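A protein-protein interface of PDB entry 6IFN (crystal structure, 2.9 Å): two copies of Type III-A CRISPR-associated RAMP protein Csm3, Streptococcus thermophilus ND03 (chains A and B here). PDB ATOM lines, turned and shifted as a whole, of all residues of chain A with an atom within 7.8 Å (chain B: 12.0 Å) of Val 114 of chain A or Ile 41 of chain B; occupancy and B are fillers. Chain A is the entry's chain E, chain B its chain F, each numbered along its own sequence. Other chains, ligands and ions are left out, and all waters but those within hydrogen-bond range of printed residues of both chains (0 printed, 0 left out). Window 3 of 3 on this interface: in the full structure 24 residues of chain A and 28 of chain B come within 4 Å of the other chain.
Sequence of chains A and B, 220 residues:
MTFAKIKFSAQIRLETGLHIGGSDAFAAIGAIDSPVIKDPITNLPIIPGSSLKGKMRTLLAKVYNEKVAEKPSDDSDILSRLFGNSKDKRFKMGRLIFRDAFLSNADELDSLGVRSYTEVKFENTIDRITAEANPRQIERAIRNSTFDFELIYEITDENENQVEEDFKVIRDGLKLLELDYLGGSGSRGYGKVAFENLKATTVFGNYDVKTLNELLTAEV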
ATOM      1  N   ASN A 105      -5.429  10.302  37.591  1.00  0.00           N
ATOM      2  CA  ASN A 105      -6.298   9.339  36.859  1.00  0.00           C
ATOM      3  C   ASN A 105      -5.639   7.966  36.651  1.00  0.00           C
ATOM      4  O   ASN A 105      -6.162   7.191  35.877  1.00  0.00           O
ATOM      5  CB  ASN A 105      -6.728   9.879  35.488  1.00  0.00           C
ATOM      6  CG  ASN A 105      -5.551  10.238  34.601  1.00  0.00           C
ATOM      7  OD1 ASN A 105      -4.409  10.167  35.045  1.00  0.00           O
ATOM      8  ND2 ASN A 105      -5.800  10.652  33.366  1.00  0.00           N
ATOM      9  N   ALA A 106      -4.572   7.628  37.388  1.00  0.00           N
ATOM     10  CA  ALA A 106      -3.904   6.302  37.257  1.00  0.00           C
ATOM     11  C   ALA A 106      -4.943   5.185  37.213  1.00  0.00           C
ATOM     12  O   ALA A 106      -4.828   4.253  36.441  1.00  0.00           O
ATOM     13  CB  ALA A 106      -2.945   6.063  38.398  1.00  0.00           C
ATOM     14  N   ASP A 107      -5.956   5.303  38.075  1.00  0.00           N
ATOM     15  CA  ASP A 107      -6.986   4.285  38.242  1.00  0.00           C
ATOM     16  C   ASP A 107      -7.899   4.292  37.015  1.00  0.00           C
ATOM     17  O   ASP A 107      -8.193   3.247  36.479  1.00  0.00           O
ATOM     18  CB  ASP A 107      -7.709   4.458  39.579  1.00  0.00           C
ATOM     19  CG  ASP A 107      -6.788   4.215  40.774  1.00  0.00           C
ATOM     20  OD1 ASP A 107      -5.896   3.325  40.669  1.00  0.00           O
ATOM     21  OD2 ASP A 107      -6.926   4.948  41.789  1.00  0.00           O
ATOM     22  N   GLU A 108      -8.312   5.476  36.566  1.00  0.00           N
ATOM     23  CA  GLU A 108      -9.102   5.613  35.346  1.00  0.00           C
ATOM     24  C   GLU A 108      -8.420   4.840  34.208  1.00  0.00           C
ATOM     25  O   GLU A 108      -9.088   4.072  33.481  1.00  0.00           O
ATOM     26  CB  GLU A 108      -9.278   7.090  34.992  1.00  0.00           C
ATOM     27  CG  GLU A 108     -10.377   7.386  33.975  1.00  0.00           C
ATOM     28  CD  GLU A 108     -10.344   8.804  33.404  1.00  0.00           C
ATOM     29  OE1 GLU A 108      -9.998   9.752  34.173  1.00  0.00           O
ATOM     30  OE2 GLU A 108     -10.651   8.965  32.177  1.00  0.00           O
ATOM     31  N   LEU A 109      -7.099   5.033  34.068  1.00  0.00           N
ATOM     32  CA  LEU A 109      -6.333   4.460  32.951  1.00  0.00           C
ATOM     33  C   LEU A 109      -6.177   2.947  33.137  1.00  0.00           C
ATOM     34  O   LEU A 109      -6.300   2.196  32.174  1.00  0.00           O
ATOM     35  CB  LEU A 109      -4.965   5.143  32.848  1.00  0.00           C
ATOM     36  CG  LEU A 109      -4.991   6.650  32.588  1.00  0.00           C
ATOM     37  CD1 LEU A 109      -3.609   7.239  32.770  1.00  0.00           C
ATOM     38  CD2 LEU A 109      -5.483   6.956  31.183  1.00  0.00           C
ATOM     39  N   ASP A 110      -5.909   2.516  34.372  1.00  0.00           N
ATOM     40  CA  ASP A 110      -5.788   1.109  34.663  1.00  0.00           C
ATOM     41  C   ASP A 110      -7.098   0.411  34.244  1.00  0.00           C
ATOM     42  O   ASP A 110      -7.075  -0.705  33.689  1.00  0.00           O
ATOM     43  CB  ASP A 110      -5.423   0.870  36.132  1.00  0.00           C
ATOM     44  CG  ASP A 110      -5.093  -0.579  36.465  1.00  0.00           C
ATOM     45  OD1 ASP A 110      -4.844  -1.325  35.525  1.00  0.00           O
ATOM     46  OD2 ASP A 110      -5.113  -0.968  37.649  1.00  0.00           O
ATOM     47  N   SER A 111      -8.230   1.081  34.497  1.00  0.00           N
ATOM     48  CA  SER A 111      -9.534   0.539  34.137  1.00  0.00           C
ATOM     49  C   SER A 111      -9.718   0.494  32.610  1.00  0.00           C
ATOM     50  O   SER A 111     -10.262  -0.477  32.085  1.00  0.00           O
ATOM     51  CB  SER A 111     -10.635   1.282  34.824  1.00  0.00           C
ATOM     52  OG  SER A 111     -10.753   0.773  36.140  1.00  0.00           O
ATOM     53  N   LEU A 112      -9.252   1.528  31.902  1.00  0.00           N
ATOM     54  CA  LEU A 112      -9.377   1.584  30.441  1.00  0.00           C
ATOM     55  C   LEU A 112      -8.508   0.512  29.768  1.00  0.00           C
ATOM     56  O   LEU A 112      -8.650   0.294  28.544  1.00  0.00           O
ATOM     57  CB  LEU A 112      -8.962   2.973  29.934  1.00  0.00           C
ATOM     58  CG  LEU A 112     -10.031   4.054  29.853  1.00  0.00           C
ATOM     59  CD1 LEU A 112      -9.503   5.241  29.056  1.00  0.00           C
ATOM     60  CD2 LEU A 112     -11.305   3.524  29.210  1.00  0.00           C
ATOM     61  N   GLY A 113      -7.585  -0.104  30.543  1.00  0.00           N
ATOM     62  CA  GLY A 113      -6.622  -1.082  30.031  1.00  0.00           C
ATOM     63  C   GLY A 113      -5.402  -0.425  29.369  1.00  0.00           C
ATOM     64  O   GLY A 113      -4.787  -0.963  28.451  1.00  0.00           O
ATOM     65  N   VAL A 114      -4.994   0.744  29.877  1.00  0.00           N
ATOM     66  CA  VAL A 114      -3.679   1.307  29.602  1.00  0.00           C
ATOM     67  C   VAL A 114      -2.647   0.532  30.434  1.00  0.00           C
ATOM     68  O   VAL A 114      -2.945   0.087  31.537  1.00  0.00           O
ATOM     69  CB  VAL A 114      -3.667   2.800  29.943  1.00  0.00           C
ATOM     70  CG1 VAL A 114      -2.382   3.454  29.494  1.00  0.00           C
ATOM     71  CG2 VAL A 114      -4.871   3.501  29.368  1.00  0.00           C
ATOM     72  N   ARG A 115      -1.425   0.391  29.918  1.00  0.00           N
ATOM     73  CA  ARG A 115      -0.402  -0.455  30.577  1.00  0.00           C
ATOM     74  C   ARG A 115       0.694   0.409  31.215  1.00  0.00           C
ATOM     75  O   ARG A 115       0.815   0.386  32.425  1.00  0.00           O
ATOM     76  CB  ARG A 115       0.150  -1.494  29.594  1.00  0.00           C
ATOM     77  CG  ARG A 115      -0.839  -2.614  29.286  1.00  0.00           C
ATOM     78  CD  ARG A 115      -0.193  -3.884  28.714  1.00  0.00           C
ATOM     79  NE  ARG A 115      -0.103  -3.916  27.253  1.00  0.00           N
ATOM     80  CZ  ARG A 115      -1.138  -4.101  26.417  1.00  0.00           C
ATOM     81  NH1 ARG A 115      -0.923  -4.249  25.120  1.00  0.00           N
ATOM     82  NH2 ARG A 115      -2.382  -4.124  26.873  1.00  0.00           N
ATOM     83  N   SER A 116       1.480   1.144  30.418  1.00  0.00           N
ATOM     84  CA  SER A 116       2.477   2.085  30.966  1.00  0.00           C
ATOM     85  C   SER A 116       1.900   3.510  30.941  1.00  0.00           C
ATOM     86  O   SER A 116       1.061   3.831  30.071  1.00  0.00           O
ATOM     87  CB  SER A 116       3.786   1.996  30.224  1.00  0.00           C
ATOM     88  N   TYR A 117       2.389   4.367  31.850  1.00  0.00           N
ATOM     89  CA  TYR A 117       1.953   5.771  31.894  1.00  0.00           C
ATOM     90  C   TYR A 117       2.969   6.676  31.199  1.00  0.00           C
ATOM     91  O   TYR A 117       2.863   7.916  31.271  1.00  0.00           O
ATOM     92  CB  TYR A 117       1.727   6.222  33.333  1.00  0.00           C
ATOM     93  CG  TYR A 117       0.717   5.372  34.046  1.00  0.00           C
ATOM     94  CD1 TYR A 117      -0.637   5.516  33.802  1.00  0.00           C
ATOM     95  CD2 TYR A 117       1.119   4.375  34.898  1.00  0.00           C
ATOM     96  CE1 TYR A 117      -1.574   4.725  34.438  1.00  0.00           C
ATOM     97  CE2 TYR A 117       0.195   3.586  35.554  1.00  0.00           C
ATOM     98  CZ  TYR A 117      -1.157   3.747  35.314  1.00  0.00           C
ATOM     99  OH  TYR A 117      -2.066   2.912  35.909  1.00  0.00           O
ATOM    100  N   THR A 118       3.943   6.052  30.532  1.00  0.00           N
ATOM    101  CA  THR A 118       4.912   6.730  29.713  1.00  0.00           C
ATOM    102  C   THR A 118       5.081   5.987  28.378  1.00  0.00           C
ATOM    103  O   THR A 118       5.105   4.780  28.334  1.00  0.00           O
ATOM    104  CB  THR A 118       6.250   6.869  30.445  1.00  0.00           C
ATOM    105  OG1 THR A 118       6.731   5.570  30.750  1.00  0.00           O
ATOM    106  CG2 THR A 118       6.169   7.645  31.741  1.00  0.00           C
ATOM    107  N   GLU A 119       5.193   6.764  27.294  1.00  0.00           N
ATOM    108  CA  GLU A 119       5.556   6.305  25.988  1.00  0.00           C
ATOM    109  C   GLU A 119       7.045   6.575  25.797  1.00  0.00           C
ATOM    110  O   GLU A 119       7.582   7.508  26.381  1.00  0.00           O
ATOM    111  CB  GLU A 119       4.694   7.005  24.924  1.00  0.00           C
ATOM    112  CG  GLU A 119       5.224   8.338  24.418  1.00  0.00           C
ATOM    113  CD  GLU A 119       4.207   9.133  23.602  1.00  0.00           C
ATOM    114  OE1 GLU A 119       3.799  10.254  24.041  1.00  0.00           O
ATOM    115  OE2 GLU A 119       3.796   8.624  22.540  1.00  0.00           O
ATOM    116  N   ILE A 142       2.452  10.017  29.133  1.00  0.00           N
ATOM    117  CA  ILE A 142       1.541   9.876  28.019  1.00  0.00           C
ATOM    118  C   ILE A 142       0.557  11.044  28.057  1.00  0.00           C
ATOM    119  O   ILE A 142       0.266  11.578  29.112  1.00  0.00           O
ATOM    120  CB  ILE A 142       0.831   8.511  28.011  1.00  0.00           C
ATOM    121  CG1 ILE A 142      -0.152   8.348  29.168  1.00  0.00           C
ATOM    122  CG2 ILE A 142       1.838   7.373  27.978  1.00  0.00           C
ATOM    123  CD1 ILE A 142      -0.871   7.014  29.155  1.00  0.00           C
ATOM    124  N   ARG A 143       0.042  11.414  26.884  1.00  0.00           N
ATOM    125  CA  ARG A 143      -0.905  12.476  26.815  1.00  0.00           C
ATOM    126  C   ARG A 143      -2.234  11.975  27.395  1.00  0.00           C
ATOM    127  O   ARG A 143      -2.517  10.808  27.411  1.00  0.00           O
ATOM    128  CB  ARG A 143      -1.007  12.994  25.383  1.00  0.00           C
ATOM    129  CG  ARG A 143      -2.300  12.641  24.664  1.00  0.00           C
ATOM    130  CD  ARG A 143      -2.328  13.307  23.299  1.00  0.00           C
ATOM    131  NE  ARG A 143      -3.639  13.801  22.902  1.00  0.00           N
ATOM    132  CZ  ARG A 143      -4.588  13.053  22.360  1.00  0.00           C
ATOM    133  NH1 ARG A 143      -5.673  13.641  21.896  1.00  0.00           N
ATOM    134  NH2 ARG A 143      -4.454  11.735  22.288  1.00  0.00           N
ATOM    135  N   ASN A 144      -3.041  12.898  27.906  1.00  0.00           N
ATOM    136  CA  ASN A 144      -4.295  12.598  28.612  1.00  0.00           C
ATOM    137  C   ASN A 144      -4.060  11.913  29.962  1.00  0.00           C
ATOM    138  O   ASN A 144      -4.991  11.452  30.558  1.00  0.00           O
ATOM    139  CB  ASN A 144      -5.286  11.817  27.763  1.00  0.00           C
ATOM    140  CG  ASN A 144      -6.060  12.797  26.924  1.00  0.00           C
ATOM    141  OD1 ASN A 144      -7.014  13.375  27.433  1.00  0.00           O
ATOM    142  ND2 ASN A 144      -5.568  13.078  25.721  1.00  0.00           N
ATOM    143  N   SER A 145      -2.835  11.952  30.486  1.00  0.00           N
ATOM    144  CA  SER A 145      -2.585  11.848  31.922  1.00  0.00           C
ATOM    145  C   SER A 145      -3.113  13.127  32.579  1.00  0.00           C
ATOM    146  O   SER A 145      -3.056  14.217  31.945  1.00  0.00           O
ATOM    147  CB  SER A 145      -1.113  11.676  32.205  1.00  0.00           C
ATOM    148  OG  SER A 145      -0.586  10.532  31.547  1.00  0.00           O
ATOM    149  N   PHE B  26       8.860  -2.031  20.059  1.00  0.00           N
ATOM    150  CA  PHE B  26       7.680  -1.662  20.844  1.00  0.00           C
ATOM    151  C   PHE B  26       6.417  -1.862  20.012  1.00  0.00           C
ATOM    152  O   PHE B  26       5.332  -1.443  20.408  1.00  0.00           O
ATOM    153  CB  PHE B  26       7.788  -0.225  21.357  1.00  0.00           C
ATOM    154  CG  PHE B  26       8.800  -0.130  22.461  1.00  0.00           C
ATOM    155  CD1 PHE B  26      10.147   0.017  22.165  1.00  0.00           C
ATOM    156  CD2 PHE B  26       8.420  -0.306  23.780  1.00  0.00           C
ATOM    157  CE1 PHE B  26      11.095   0.043  23.178  1.00  0.00           C
ATOM    158  CE2 PHE B  26       9.371  -0.273  24.788  1.00  0.00           C
ATOM    159  CZ  PHE B  26      10.706  -0.109  24.486  1.00  0.00           C
ATOM    160  N   VAL B  36       3.668   2.667  12.373  1.00  0.00           N
ATOM    161  CA  VAL B  36       3.678   4.127  12.365  1.00  0.00           C
ATOM    162  C   VAL B  36       3.478   4.639  13.796  1.00  0.00           C
ATOM    163  O   VAL B  36       2.872   3.996  14.595  1.00  0.00           O
ATOM    164  CB  VAL B  36       2.605   4.669  11.416  1.00  0.00           C
ATOM    165  CG1 VAL B  36       2.735   4.061  10.032  1.00  0.00           C
ATOM    166  CG2 VAL B  36       1.215   4.435  11.984  1.00  0.00           C
ATOM    167  N   ILE B  37       3.991   5.830  14.079  1.00  0.00           N
ATOM    168  CA  ILE B  37       4.004   6.424  15.417  1.00  0.00           C
ATOM    169  C   ILE B  37       2.554   6.672  15.828  1.00  0.00           C
ATOM    170  O   ILE B  37       1.763   7.252  15.031  1.00  0.00           O
ATOM    171  CB  ILE B  37       4.823   7.736  15.453  1.00  0.00           C
ATOM    172  CG1 ILE B  37       4.887   8.345  16.858  1.00  0.00           C
ATOM    173  CG2 ILE B  37       4.300   8.762  14.455  1.00  0.00           C
ATOM    174  CD1 ILE B  37       5.988   7.765  17.722  1.00  0.00           C
ATOM    175  N   LYS B  38       2.205   6.226  17.040  1.00  0.00           N
ATOM    176  CA  LYS B  38       0.809   6.258  17.490  1.00  0.00           C
ATOM    177  C   LYS B  38       0.711   6.828  18.906  1.00  0.00           C
ATOM    178  O   LYS B  38       1.562   6.599  19.726  1.00  0.00           O
ATOM    179  CB  LYS B  38       0.176   4.865  17.447  1.00  0.00           C
ATOM    180  CG  LYS B  38       0.263   4.162  16.100  1.00  0.00           C
ATOM    181  CD  LYS B  38      -0.525   2.876  15.997  1.00  0.00           C
ATOM    182  CE  LYS B  38      -0.492   2.277  14.598  1.00  0.00           C
ATOM    183  NZ  LYS B  38       0.752   1.521  14.360  1.00  0.00           N
ATOM    184  N   ASP B  39      -0.361   7.577  19.152  1.00  0.00           N
ATOM    185  CA  ASP B  39      -0.695   8.075  20.466  1.00  0.00           C
ATOM    186  C   ASP B  39      -1.055   6.901  21.361  1.00  0.00           C
ATOM    187  O   ASP B  39      -1.977   6.168  21.054  1.00  0.00           O
ATOM    188  CB  ASP B  39      -1.873   9.050  20.416  1.00  0.00           C
ATOM    189  CG  ASP B  39      -2.543   9.286  21.764  1.00  0.00           C
ATOM    190  OD1 ASP B  39      -1.851   9.703  22.720  1.00  0.00           O
ATOM    191  OD2 ASP B  39      -3.752   9.104  21.839  1.00  0.00           O
ATOM    192  N   PRO B  40      -0.378   6.709  22.508  1.00  0.00           N
ATOM    193  CA  PRO B  40      -0.476   5.469  23.266  1.00  0.00           C
ATOM    194  C   PRO B  40      -1.880   5.160  23.788  1.00  0.00           C
ATOM    195  O   PRO B  40      -2.225   4.006  23.878  1.00  0.00           O
ATOM    196  CB  PRO B  40       0.504   5.653  24.442  1.00  0.00           C
ATOM    197  CG  PRO B  40       0.667   7.129  24.568  1.00  0.00           C
ATOM    198  CD  PRO B  40       0.540   7.655  23.146  1.00  0.00           C
ATOM    199  N   ILE B  41      -2.659   6.184  24.132  1.00  0.00           N
ATOM    200  CA  ILE B  41      -3.943   5.953  24.798  1.00  0.00           C
ATOM    201  C   ILE B  41      -4.995   5.496  23.776  1.00  0.00           C
ATOM    202  O   ILE B  41      -5.753   4.588  24.049  1.00  0.00           O
ATOM    203  CB  ILE B  41      -4.403   7.194  25.594  1.00  0.00           C
ATOM    204  CG1 ILE B  41      -5.684   6.904  26.369  1.00  0.00           C
ATOM    205  CG2 ILE B  41      -4.592   8.426  24.712  1.00  0.00           C
ATOM    206  CD1 ILE B  41      -5.656   5.604  27.086  1.00  0.00           C
ATOM    207  N   THR B  42      -5.017   6.122  22.595  1.00  0.00           N
ATOM    208  CA  THR B  42      -6.024   5.854  21.555  1.00  0.00           C
ATOM    209  C   THR B  42      -5.490   4.920  20.459  1.00  0.00           C
ATOM    210  O   THR B  42      -6.247   4.483  19.598  1.00  0.00           O
ATOM    211  CB  THR B  42      -6.509   7.155  20.898  1.00  0.00           C
ATOM    212  OG1 THR B  42      -5.455   7.739  20.124  1.00  0.00           O
ATOM    213  CG2 THR B  42      -7.017   8.161  21.906  1.00  0.00           C
ATOM    214  N   ASN B  43      -4.181   4.669  20.455  1.00  0.00           N
ATOM    215  CA  ASN B  43      -3.516   3.853  19.438  1.00  0.00           C
ATOM    216  C   ASN B  43      -3.790   4.404  18.029  1.00  0.00           C
ATOM    217  O   ASN B  43      -3.643   3.673  17.070  1.00  0.00           O
ATOM    218  CB  ASN B  43      -3.939   2.387  19.586  1.00  0.00           C
ATOM    219  CG  ASN B  43      -2.976   1.390  18.980  1.00  0.00           C
ATOM    220  OD1 ASN B  43      -1.823   1.715  18.672  1.00  0.00           O
ATOM    221  ND2 ASN B  43      -3.442   0.151  18.860  1.00  0.00           N
ATOM    222  N   LEU B  44      -4.105   5.696  17.912  1.00  0.00           N
ATOM    223  CA  LEU B  44      -4.313   6.319  16.624  1.00  0.00           C
ATOM    224  C   LEU B  44      -3.009   6.908  16.111  1.00  0.00           C
ATOM    225  O   LEU B  44      -2.124   7.248  16.886  1.00  0.00           O
ATOM    226  CB  LEU B  44      -5.361   7.422  16.771  1.00  0.00           C
ATOM    227  CG  LEU B  44      -6.746   6.946  17.175  1.00  0.00           C
ATOM    228  CD1 LEU B  44      -7.717   8.117  17.197  1.00  0.00           C
ATOM    229  CD2 LEU B  44      -7.226   5.845  16.237  1.00  0.00           C
ATOM    230  N   PRO B  45      -2.855   7.082  14.789  1.00  0.00           N
ATOM    231  CA  PRO B  45      -1.725   7.821  14.252  1.00  0.00           C
ATOM    232  C   PRO B  45      -1.692   9.248  14.800  1.00  0.00           C
ATOM    233  O   PRO B  45      -2.727   9.847  15.078  1.00  0.00           O
ATOM    234  CB  PRO B  45      -1.957   7.851  12.738  1.00  0.00           C
ATOM    235  CG  PRO B  45      -3.434   7.543  12.584  1.00  0.00           C
ATOM    236  CD  PRO B  45      -3.750   6.602  13.733  1.00  0.00           C
ATOM    237  N   ILE B  46      -0.463   9.748  14.912  1.00  0.00           N
ATOM    238  CA  ILE B  46      -0.121  11.044  15.430  1.00  0.00           C
ATOM    239  C   ILE B  46       0.873  11.644  14.428  1.00  0.00           C
ATOM    240  O   ILE B  46       1.666  10.891  13.837  1.00  0.00           O
ATOM    241  CB  ILE B  46       0.461  10.864  16.847  1.00  0.00           C
ATOM    242  CG1 ILE B  46       0.604  12.164  17.620  1.00  0.00           C
ATOM    243  CG2 ILE B  46       1.816  10.188  16.817  1.00  0.00           C
ATOM    244  CD1 ILE B  46       1.492  12.009  18.858  1.00  0.00           C
ATOM    245  N   ASP B 100       2.314  18.380  18.514  1.00  0.00           N
ATOM    246  CA  ASP B 100       1.864  17.088  18.076  1.00  0.00           C
ATOM    247  C   ASP B 100       0.439  17.260  17.524  1.00  0.00           C
ATOM    248  O   ASP B 100      -0.430  17.848  18.180  1.00  0.00           O
ATOM    249  CB  ASP B 100       1.865  16.054  19.208  1.00  0.00           C
ATOM    250  CG  ASP B 100       3.230  15.519  19.627  1.00  0.00           C
ATOM    251  OD1 ASP B 100       4.277  15.917  18.983  1.00  0.00           O
ATOM    252  OD2 ASP B 100       3.237  14.709  20.623  1.00  0.00           O
ATOM    253  N   ALA B 101       0.214  16.778  16.298  1.00  0.00           N
ATOM    254  CA  ALA B 101      -1.066  16.861  15.654  1.00  0.00           C
ATOM    255  C   ALA B 101      -1.794  15.528  15.820  1.00  0.00           C
ATOM    256  O   ALA B 101      -1.189  14.474  15.688  1.00  0.00           O
ATOM    257  CB  ALA B 101      -0.866  17.225  14.212  1.00  0.00           C
ATOM    258  N   PHE B 102      -3.096  15.595  16.108  1.00  0.00           N
ATOM    259  CA  PHE B 102      -3.875  14.405  16.407  1.00  0.00           C
ATOM    260  C   PHE B 102      -5.016  14.285  15.406  1.00  0.00           C
ATOM    261  O   PHE B 102      -5.463  15.271  14.817  1.00  0.00           O
ATOM    262  CB  PHE B 102      -4.414  14.432  17.836  1.00  0.00           C
ATOM    263  CG  PHE B 102      -3.317  14.480  18.857  1.00  0.00           C
ATOM    264  CD1 PHE B 102      -2.701  13.319  19.274  1.00  0.00           C
ATOM    265  CD2 PHE B 102      -2.851  15.694  19.330  1.00  0.00           C
ATOM    266  CE1 PHE B 102      -1.669  13.369  20.196  1.00  0.00           C
ATOM    267  CE2 PHE B 102      -1.820  15.740  20.249  1.00  0.00           C
ATOM    268  CZ  PHE B 102      -1.220  14.580  20.670  1.00  0.00           C
ATOM    269  N   LEU B 103      -5.489  13.048  15.255  1.00  0.00           N
ATOM    270  CA  LEU B 103      -6.494  12.718  14.287  1.00  0.00           C
ATOM    271  C   LEU B 103      -7.799  13.416  14.688  1.00  0.00           C
ATOM    272  O   LEU B 103      -8.328  13.151  15.779  1.00  0.00           O
ATOM    273  CB  LEU B 103      -6.654  11.191  14.264  1.00  0.00           C
ATOM    274  CG  LEU B 103      -7.588  10.615  13.194  1.00  0.00           C
ATOM    275  CD1 LEU B 103      -6.843  10.411  11.875  1.00  0.00           C
ATOM    276  CD2 LEU B 103      -8.242   9.315  13.666  1.00  0.00           C
ATOM    277  N   ALA B 106     -11.898  11.204  13.103  1.00  0.00           N
ATOM    278  CA  ALA B 106     -12.284   9.830  13.477  1.00  0.00           C
ATOM    279  C   ALA B 106     -13.787   9.604  13.268  1.00  0.00           C
ATOM    280  O   ALA B 106     -14.170   8.546  12.810  1.00  0.00           O
ATOM    281  CB  ALA B 106     -11.910   9.549  14.913  1.00  0.00           C
ATOM    282  N   TYR B 117      -7.692   2.771  10.819  1.00  0.00           N
ATOM    283  CA  TYR B 117      -7.177   4.111  10.537  1.00  0.00           C
ATOM    284  C   TYR B 117      -5.820   4.028   9.843  1.00  0.00           C
ATOM    285  O   TYR B 117      -5.232   5.076   9.536  1.00  0.00           O
ATOM    286  CB  TYR B 117      -7.111   4.930  11.828  1.00  0.00           C
ATOM    287  CG  TYR B 117      -8.455   5.092  12.479  1.00  0.00           C
ATOM    288  CD1 TYR B 117      -9.379   6.002  11.993  1.00  0.00           C
ATOM    289  CD2 TYR B 117      -8.820   4.292  13.539  1.00  0.00           C
ATOM    290  CE1 TYR B 117     -10.619   6.160  12.586  1.00  0.00           C
ATOM    291  CE2 TYR B 117     -10.059   4.425  14.141  1.00  0.00           C
ATOM    292  CZ  TYR B 117     -10.958   5.367  13.671  1.00  0.00           C
ATOM    293  OH  TYR B 117     -12.170   5.503  14.287  1.00  0.00           O
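No residue of chain B comes within 4 Å of Leu 109 of chain A.
Leu 112 of chain A touches none of the printed residues of chain B.
No residue of chain B comes within 4 Å of Gly 113 of chain A.
Val 114 of chain A touches just one residue of chain B: Ile 41 (3.2 Å).
No residue of chain B comes within 4 Å of Arg 115 of chain A.
No residue of chain B comes within 4 Å of Ser 116 of chain A.
No residue of chain B comes within 4 Å of Tyr 117 of chain A.
Printed residues of chain B within 4 Å of Glu 119 of chain A: Pro 40.
Of the printed residues of chain B, Ile 142 of chain A touches Pro 40 (3.6 Å).
Arg 143 of chain A touches just these residues of chain B: Asp 39 (2.8 Å) and Phe 102 (3.1 Å).
Ser 145 of chain A touches none of the printed residues of chain B.
Pro 40 of chain B touches two residues of chain A.
Ile 41 of chain B touches just one residue of chain A: Val 114.
Of the printed residues of chain A, Phe 102 of chain B touches Arg 143.
Tyr 117 of chain B touches none of the printed residues of chain A.
The nearest residue of chain A that does not touch Ile 41 of chain B is Arg 143 of chain A (4.1 Å).
The side-chain hydroxyl (OG1) of Thr 42 of chain B is in hydrogen-bond range of the side-chain carboxylate (OD2) of Asp 39 of chain B, at 2.8 Å.
N of Asp 39 of chain B lies within hydrogen-bond range of O of Leu 44 of chain B (2.9 Å).
The backbone NH of Val 114 of chain A sits at hydrogen-bond distance from the backbone carbonyl oxygen of Leu 109 of chain A (3.0 Å).
The backbone NH (N) of Ile 142 of chain A is in hydrogen-bond range of the backbone carbonyl oxygen (O) of Tyr 117 of chain A (3.0 Å).
O of Ile 142 of chain A lies within hydrogen-bond range of OG of Ser 145 of chain A, 2.8 Å away.
ND2 of Asn 144 of chain A sits close to NE of Arg 143 of chain A (3.5 Å).
2 positions are printed for both chains.
OD2 of Asp 39 of chain B is in salt-bridge range of NH2 of Arg 143 of chain A.
Ile 41 of chain B touches Val 114 of chain A.
Pro 40 of chain B touches Glu 119 of chain A (CD to OE2, 3.5 Å).
Ile 142 of chain A touches Pro 40 of chain B.
Arg 143 of chain A touches Phe 102 of chain B (CD to CZ, 3.1 Å).
Of the 19 printed residues of chain A, 4 touch a printed residue of chain B.
Printed residues of chain A that touch a printed residue of chain B: Val 114, Glu 119, Ile 142 and Arg 143.
Hydrophobic or aromatic side chains of chain A within 4 Å of the printed part of chain B: Val 114 and Ile 142.
Among the printed residues, 5 pairs touch across the chains.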
